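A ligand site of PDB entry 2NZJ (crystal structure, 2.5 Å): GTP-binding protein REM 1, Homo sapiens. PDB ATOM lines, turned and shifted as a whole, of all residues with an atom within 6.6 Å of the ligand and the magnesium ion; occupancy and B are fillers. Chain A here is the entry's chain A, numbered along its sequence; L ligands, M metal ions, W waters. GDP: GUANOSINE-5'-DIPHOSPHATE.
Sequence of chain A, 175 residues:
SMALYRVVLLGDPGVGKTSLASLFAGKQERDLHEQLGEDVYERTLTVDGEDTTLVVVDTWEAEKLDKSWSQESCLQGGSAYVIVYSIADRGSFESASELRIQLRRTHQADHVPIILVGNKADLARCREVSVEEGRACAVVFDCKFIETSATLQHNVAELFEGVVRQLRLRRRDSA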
ATOM      1  N   GLY A  11       3.142  24.386  17.351  1.00  0.00           N
ATOM      2  CA  GLY A  11       2.510  23.179  16.857  1.00  0.00           C
ATOM      3  C   GLY A  11       1.366  22.709  17.733  1.00  0.00           C
ATOM      4  O   GLY A  11       1.272  23.068  18.909  1.00  0.00           O
ATOM      5  N   ASP A  12       0.505  21.860  17.177  1.00  0.00           N
ATOM      6  CA  ASP A  12      -0.613  21.280  17.917  1.00  0.00           C
ATOM      7  C   ASP A  12      -0.195  20.493  19.167  1.00  0.00           C
ATOM      8  O   ASP A  12       0.934  20.003  19.260  1.00  0.00           O
ATOM      9  CB  ASP A  12      -1.411  20.349  16.998  1.00  0.00           C
ATOM     10  CG  ASP A  12      -2.345  21.099  16.068  1.00  0.00           C
ATOM     11  OD1 ASP A  12      -2.426  22.350  16.136  1.00  0.00           O
ATOM     12  OD2 ASP A  12      -3.031  20.436  15.266  1.00  0.00           O
ATOM     13  N   PRO A  13      -1.116  20.355  20.133  1.00  0.00           N
ATOM     14  CA  PRO A  13      -0.812  19.530  21.305  1.00  0.00           C
ATOM     15  C   PRO A  13      -0.536  18.080  20.928  1.00  0.00           C
ATOM     16  O   PRO A  13      -1.193  17.550  20.023  1.00  0.00           O
ATOM     17  CB  PRO A  13      -2.088  19.599  22.141  1.00  0.00           C
ATOM     18  CG  PRO A  13      -2.930  20.687  21.550  1.00  0.00           C
ATOM     19  CD  PRO A  13      -2.462  20.942  20.167  1.00  0.00           C
ATOM     20  N   GLY A  14       0.431  17.459  21.597  1.00  0.00           N
ATOM     21  CA  GLY A  14       0.721  16.046  21.421  1.00  0.00           C
ATOM     22  C   GLY A  14       1.774  15.695  20.388  1.00  0.00           C
ATOM     23  O   GLY A  14       2.148  14.530  20.262  1.00  0.00           O
ATOM     24  N   VAL A  15       2.298  16.692  19.685  1.00  0.00           N
ATOM     25  CA  VAL A  15       3.275  16.414  18.637  1.00  0.00           C
ATOM     26  C   VAL A  15       4.683  16.185  19.202  1.00  0.00           C
ATOM     27  O   VAL A  15       5.551  15.650  18.492  1.00  0.00           O
ATOM     28  CB  VAL A  15       3.259  17.511  17.545  1.00  0.00           C
ATOM     29  CG1 VAL A  15       1.936  17.459  16.774  1.00  0.00           C
ATOM     30  CG2 VAL A  15       3.503  18.896  18.123  1.00  0.00           C
ATOM     31  N   GLY A  16       4.923  16.596  20.440  1.00  0.00           N
ATOM     32  CA  GLY A  16       6.234  16.381  21.100  1.00  0.00           C
ATOM     33  C   GLY A  16       7.087  17.622  21.337  1.00  0.00           C
ATOM     34  O   GLY A  16       8.306  17.540  21.435  1.00  0.00           O
ATOM     35  N   LYS A  17       6.438  18.786  21.438  1.00  0.00           N
ATOM     36  CA  LYS A  17       7.134  20.065  21.654  1.00  0.00           C
ATOM     37  C   LYS A  17       7.884  20.099  22.993  1.00  0.00           C
ATOM     38  O   LYS A  17       9.076  20.420  23.034  1.00  0.00           O
ATOM     39  CB  LYS A  17       6.130  21.232  21.609  1.00  0.00           C
ATOM     40  CG  LYS A  17       5.471  21.415  20.265  1.00  0.00           C
ATOM     41  CD  LYS A  17       4.709  22.728  20.189  1.00  0.00           C
ATOM     42  CE  LYS A  17       3.471  22.714  21.099  1.00  0.00           C
ATOM     43  NZ  LYS A  17       2.505  21.639  20.799  1.00  0.00           N
ATOM     44  N   THR A  18       7.180  19.762  24.068  1.00  0.00           N
ATOM     45  CA  THR A  18       7.804  19.726  25.366  1.00  0.00           C
ATOM     46  C   THR A  18       8.918  18.673  25.444  1.00  0.00           C
ATOM     47  O   THR A  18       9.943  18.894  26.079  1.00  0.00           O
ATOM     48  CB  THR A  18       6.741  19.556  26.496  1.00  0.00           C
ATOM     49  OG1 THR A  18       5.851  20.682  26.478  1.00  0.00           O
ATOM     50  CG2 THR A  18       7.405  19.443  27.920  1.00  0.00           C
ATOM     51  N   SER A  19       8.753  17.551  24.782  1.00  0.00           N
ATOM     52  CA  SER A  19       9.780  16.518  24.774  1.00  0.00           C
ATOM     53  C   SER A  19      11.073  17.010  24.107  1.00  0.00           C
ATOM     54  O   SER A  19      12.164  16.846  24.658  1.00  0.00           O
ATOM     55  CB  SER A  19       9.274  15.265  24.086  1.00  0.00           C
ATOM     56  OG  SER A  19       8.047  14.843  24.664  1.00  0.00           O
ATOM     57  N   LEU A  20      10.932  17.654  22.944  1.00  0.00           N
ATOM     58  CA  LEU A  20      12.065  18.217  22.236  1.00  0.00           C
ATOM     59  C   LEU A  20      12.763  19.275  23.093  1.00  0.00           C
ATOM     60  O   LEU A  20      13.988  19.343  23.154  1.00  0.00           O
ATOM     61  CB  LEU A  20      11.611  18.826  20.904  1.00  0.00           C
ATOM     62  CG  LEU A  20      11.027  17.855  19.851  1.00  0.00           C
ATOM     63  CD1 LEU A  20      10.448  18.621  18.694  1.00  0.00           C
ATOM     64  CD2 LEU A  20      12.030  16.847  19.342  1.00  0.00           C
ATOM     65  N   ASP A  58       8.428  27.270  25.121  1.00  0.00           N
ATOM     66  CA  ASP A  58       7.469  26.180  24.918  1.00  0.00           C
ATOM     67  C   ASP A  58       6.141  26.505  25.579  1.00  0.00           C
ATOM     68  O   ASP A  58       5.647  25.757  26.414  1.00  0.00           O
ATOM     69  CB  ASP A  58       8.040  24.881  25.499  1.00  0.00           C
ATOM     70  CG  ASP A  58       7.064  23.729  25.415  1.00  0.00           C
ATOM     71  OD1 ASP A  58       6.316  23.678  24.412  1.00  0.00           O
ATOM     72  OD2 ASP A  58       7.056  22.873  26.360  1.00  0.00           O
ATOM     73  N   VAL A  84       6.526  22.304  14.814  1.00  0.00           N
ATOM     74  CA  VAL A  84       6.597  20.850  14.961  1.00  0.00           C
ATOM     75  C   VAL A  84       5.259  20.224  14.632  1.00  0.00           C
ATOM     76  O   VAL A  84       4.230  20.729  15.051  1.00  0.00           O
ATOM     77  CB  VAL A  84       6.943  20.485  16.398  1.00  0.00           C
ATOM     78  CG1 VAL A  84       6.969  18.960  16.601  1.00  0.00           C
ATOM     79  CG2 VAL A  84       8.268  21.159  16.792  1.00  0.00           C
ATOM     80  N   ASN A 119       8.196  15.308  13.828  1.00  0.00           N
ATOM     81  CA  ASN A 119       8.578  14.520  14.998  1.00  0.00           C
ATOM     82  C   ASN A 119       7.862  13.157  15.011  1.00  0.00           C
ATOM     83  O   ASN A 119       6.951  12.911  14.221  1.00  0.00           O
ATOM     84  CB  ASN A 119       8.273  15.302  16.289  1.00  0.00           C
ATOM     85  CG  ASN A 119       8.890  14.673  17.519  1.00  0.00           C
ATOM     86  OD1 ASN A 119      10.026  14.159  17.478  1.00  0.00           O
ATOM     87  ND2 ASN A 119       8.157  14.716  18.635  1.00  0.00           N
ATOM     88  N   LYS A 120       8.295  12.278  15.889  1.00  0.00           N
ATOM     89  CA  LYS A 120       7.792  10.900  15.984  1.00  0.00           C
ATOM     90  C   LYS A 120       8.148  10.038  14.762  1.00  0.00           C
ATOM     91  O   LYS A 120       7.390   9.145  14.390  1.00  0.00           O
ATOM     92  CB  LYS A 120       6.286  10.875  16.253  1.00  0.00           C
ATOM     93  CG  LYS A 120       5.838  11.835  17.359  1.00  0.00           C
ATOM     94  CD  LYS A 120       4.604  11.309  18.092  1.00  0.00           C
ATOM     95  CE  LYS A 120       4.104  12.291  19.170  1.00  0.00           C
ATOM     96  NZ  LYS A 120       2.817  11.811  19.794  1.00  0.00           N
ATOM     97  N   ALA A 121       9.325  10.288  14.170  1.00  0.00           N
ATOM     98  CA  ALA A 121       9.873   9.498  13.044  1.00  0.00           C
ATOM     99  C   ALA A 121       9.976   8.017  13.331  1.00  0.00           C
ATOM    100  O   ALA A 121       9.994   7.212  12.412  1.00  0.00           O
ATOM    101  CB  ALA A 121      11.279  10.026  12.643  1.00  0.00           C
ATOM    102  N   ASP A 122      10.095   7.658  14.605  1.00  0.00           N
ATOM    103  CA  ASP A 122      10.161   6.242  15.023  1.00  0.00           C
ATOM    104  C   ASP A 122       8.861   5.487  14.817  1.00  0.00           C
ATOM    105  O   ASP A 122       8.841   4.243  14.807  1.00  0.00           O
ATOM    106  CB  ASP A 122      10.520   6.164  16.497  1.00  0.00           C
ATOM    107  CG  ASP A 122       9.590   7.006  17.357  1.00  0.00           C
ATOM    108  OD1 ASP A 122       8.841   6.419  18.152  1.00  0.00           O
ATOM    109  OD2 ASP A 122       9.588   8.258  17.202  1.00  0.00           O
ATOM    110  N   LEU A 123       7.753   6.208  14.696  1.00  0.00           N
ATOM    111  CA  LEU A 123       6.450   5.570  14.441  1.00  0.00           C
ATOM    112  C   LEU A 123       6.308   5.336  12.949  1.00  0.00           C
ATOM    113  O   LEU A 123       5.282   5.649  12.359  1.00  0.00           O
ATOM    114  CB  LEU A 123       5.322   6.462  14.958  1.00  0.00           C
ATOM    115  CG  LEU A 123       5.389   6.782  16.439  1.00  0.00           C
ATOM    116  CD1 LEU A 123       4.168   7.549  16.864  1.00  0.00           C
ATOM    117  CD2 LEU A 123       5.530   5.497  17.221  1.00  0.00           C
ATOM    118  N   THR A 148      12.631  14.240  13.298  1.00  0.00           N
ATOM    119  CA  THR A 148      13.243  13.875  14.550  1.00  0.00           C
ATOM    120  C   THR A 148      12.435  12.801  15.254  1.00  0.00           C
ATOM    121  O   THR A 148      11.312  12.475  14.835  1.00  0.00           O
ATOM    122  CB  THR A 148      13.353  15.082  15.467  1.00  0.00           C
ATOM    123  OG1 THR A 148      12.048  15.516  15.874  1.00  0.00           O
ATOM    124  CG2 THR A 148      14.076  16.222  14.761  1.00  0.00           C
ATOM    125  N   SER A 149      13.036  12.244  16.299  1.00  0.00           N
ATOM    126  CA  SER A 149      12.324  11.454  17.289  1.00  0.00           C
ATOM    127  C   SER A 149      12.894  11.804  18.667  1.00  0.00           C
ATOM    128  O   SER A 149      14.084  11.614  18.915  1.00  0.00           O
ATOM    129  CB  SER A 149      12.426   9.952  17.020  1.00  0.00           C
ATOM    130  OG  SER A 149      11.944   9.184  18.113  1.00  0.00           O
ATOM    131  N   ALA A 150      12.042  12.281  19.568  1.00  0.00           N
ATOM    132  CA  ALA A 150      12.464  12.566  20.929  1.00  0.00           C
ATOM    133  C   ALA A 150      12.677  11.280  21.740  1.00  0.00           C
ATOM    134  O   ALA A 150      13.497  11.256  22.664  1.00  0.00           O
ATOM    135  CB  ALA A 150      11.456  13.468  21.615  1.00  0.00           C
ATOM    136  N   THR A 151      11.931  10.220  21.425  1.00  0.00           N
ATOM    137  CA  THR A 151      12.030   8.976  22.208  1.00  0.00           C
ATOM    138  C   THR A 151      13.250   8.124  21.814  1.00  0.00           C
ATOM    139  O   THR A 151      13.771   7.385  22.651  1.00  0.00           O
ATOM    140  CB  THR A 151      10.762   8.115  22.092  1.00  0.00           C
ATOM    141  OG1 THR A 151      10.548   7.772  20.721  1.00  0.00           O
ATOM    142  CG2 THR A 151       9.550   8.881  22.584  1.00  0.00           C
ATOM    143  N   LEU A 152      13.680   8.212  20.557  1.00  0.00           N
ATOM    144  CA  LEU A 152      14.950   7.591  20.134  1.00  0.00           C
ATOM    145  C   LEU A 152      16.120   8.546  20.242  1.00  0.00           C
ATOM    146  O   LEU A 152      17.261   8.168  19.992  1.00  0.00           O
ATOM    147  CB  LEU A 152      14.888   7.128  18.676  1.00  0.00           C
ATOM    148  CG  LEU A 152      14.263   5.809  18.305  1.00  0.00           C
ATOM    149  CD1 LEU A 152      14.767   5.523  16.907  1.00  0.00           C
ATOM    150  CD2 LEU A 152      14.593   4.646  19.279  1.00  0.00           C
HETATM  151  PB  GDP L   1       3.544  18.597  23.299  1.00  0.00           P
HETATM  152  O1B GDP L   1       3.689  19.009  21.856  1.00  0.00           O
HETATM  153  O2B GDP L   1       4.439  19.327  24.223  1.00  0.00           O
HETATM  154  O3B GDP L   1       2.090  18.860  23.650  1.00  0.00           O
HETATM  155  O3A GDP L   1       3.856  17.042  23.259  1.00  0.00           O
HETATM  156  PA  GDP L   1       4.595  16.327  24.479  1.00  0.00           P
HETATM  157  O1A GDP L   1       3.908  16.699  25.758  1.00  0.00           O
HETATM  158  O2A GDP L   1       6.063  16.637  24.505  1.00  0.00           O
HETATM  159  O5' GDP L   1       4.437  14.792  24.066  1.00  0.00           O
HETATM  160  C5' GDP L   1       3.162  14.214  23.780  1.00  0.00           C
HETATM  161  C4' GDP L   1       3.293  12.696  23.859  1.00  0.00           C
HETATM  162  O4' GDP L   1       3.980  12.179  22.676  1.00  0.00           O
HETATM  163  C3' GDP L   1       4.113  12.234  25.083  1.00  0.00           C
HETATM  164  O3' GDP L   1       3.521  11.099  25.737  1.00  0.00           O
HETATM  165  C2' GDP L   1       5.455  11.834  24.499  1.00  0.00           C
HETATM  166  O2' GDP L   1       6.085  10.771  25.205  1.00  0.00           O
HETATM  167  C1' GDP L   1       5.142  11.440  23.063  1.00  0.00           C
HETATM  168  N9  GDP L   1       6.242  11.790  22.147  1.00  0.00           N
HETATM  169  C8  GDP L   1       6.884  12.986  22.013  1.00  0.00           C
HETATM  170  N7  GDP L   1       7.835  12.932  21.037  1.00  0.00           N
HETATM  171  C5  GDP L   1       7.780  11.706  20.539  1.00  0.00           C
HETATM  172  C6  GDP L   1       8.512  10.954  19.520  1.00  0.00           C
HETATM  173  O6  GDP L   1       9.418  11.545  18.887  1.00  0.00           O
HETATM  174  N1  GDP L   1       8.163   9.678  19.301  1.00  0.00           N
HETATM  175  C2  GDP L   1       7.186   9.052  19.996  1.00  0.00           C
HETATM  176  N2  GDP L   1       6.856   7.760  19.761  1.00  0.00           N
HETATM  177  N3  GDP L   1       6.500   9.683  20.972  1.00  0.00           N
HETATM  178  C4  GDP L   1       6.745  10.967  21.263  1.00  0.00           C
HETATM  179 MG    MG M   1       3.785  20.370  25.968  1.00  0.00          MG
HETATM  180  O   HOH W   1       3.389  21.582  27.565  1.00  0.00           O
HETATM  181  O   HOH W   2       2.021  20.739  25.432  1.00  0.00           O
HETATM  182  O   HOH W   3       3.633  18.874  26.973  1.00  0.00           O
HETATM  183  O   HOH W   4       4.074  22.157  25.032  1.00  0.00           O
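OG1 of Thr 18 sits close to OD2 of Asp 58, 2.5 Å away.
The side-chain amide oxygen of Asn 119 sits at hydrogen-bond distance from the backbone NH of Ala 150 (3.5 Å).
OD1 of Asp 122 is in hydrogen-bond range of OG1 of Thr 151.
NZ of Lys 120 sits at hydrogen-bond distance from O of Gly 14 (2.8 Å).
ND2 of Asn 119 sits at hydrogen-bond distance from O of Val 15.
The backbone NH (N) of Lys 120 is in hydrogen-bond range of the backbone carbonyl oxygen (O) of Thr 148.
OG1 of Thr 151 sits at hydrogen-bond distance from OG of Ser 149 (3.3 Å).
N of Leu 152 sits at hydrogen-bond distance from OG of Ser 149 (3.2 Å).
Within 4 Å of the magnesium ion: Thr 18.
The nearest printed residue that does not touch the magnesium ion is Asp 58 (4.1 Å).
An oxygen (O2A) of the ligand is in hydrogen-bond range of the backbone NH of Thr 18 (3.3 Å).
An oxygen (O2A) of the ligand sits at hydrogen-bond distance from the backbone NH (N) of Ser 19, at 2.9 Å.
The side-chain hydroxyl of Ser 19 lies within hydrogen-bond range of an oxygen (O2A) of the ligand (2.7 Å).
N of Lys 17 is in hydrogen-bond range of O1B of the ligand, 2.8 Å away.
NZ of Lys 17 is in salt-bridge range of O1B of the ligand (3.1 Å).
The backbone NH (N) of Ala 150 lies within hydrogen-bond range of an oxygen (O6) of the ligand, 2.8 Å away.
A nitrogen (N2) of the ligand is in hydrogen-bond range of the side-chain carboxylate (OD1) of Asp 122, 2.9 Å away.
N of Gly 14 is in hydrogen-bond range of O3B of the ligand.
The side-chain amide nitrogen (ND2) of Asn 119 is in hydrogen-bond range of a nitrogen (N7) of the ligand, 3.0 Å away.
N of Gly 16 sits at hydrogen-bond distance from O3A of the ligand, at 3.0 Å.
The backbone NH of Lys 120 sits at hydrogen-bond distance from an oxygen (O6) of the ligand.
The side-chain amino group (NZ) of Lys 120 is in hydrogen-bond range of an oxygen (O4') of the ligand, at 3.1 Å.
N1 of the ligand lies within hydrogen-bond range of OG1 of Thr 151 (3.4 Å).
N of Val 15 lies within hydrogen-bond range of O1B of the ligand (3.5 Å).
Residues that only touch the ligand: Ser 149 (3.3 Å), Leu 123 (3.7 Å), Pro 13 (3.8 Å) and Asp 12 (3.9 Å).
Hydrophobic or aromatic side chains that line the ligand: Val 15, Leu 123 and Ala 150.
Within 4 Å of the ligand: Asp 12, Pro 13, Gly 14, Val 15, Gly 16, Lys 17, Thr 18, Ser 19, Asn 119, Lys 120, Asp 122, Leu 123, Ser 149, Ala 150 and Thr 151.
The nearest printed residue that does not touch the ligand is Thr 148 (4.6 Å).
The magnesium ion is bound by water W3, water W2, water W4, water W1, an oxygen (O2B) of the ligand and the side-chain hydroxyl of Thr 18.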
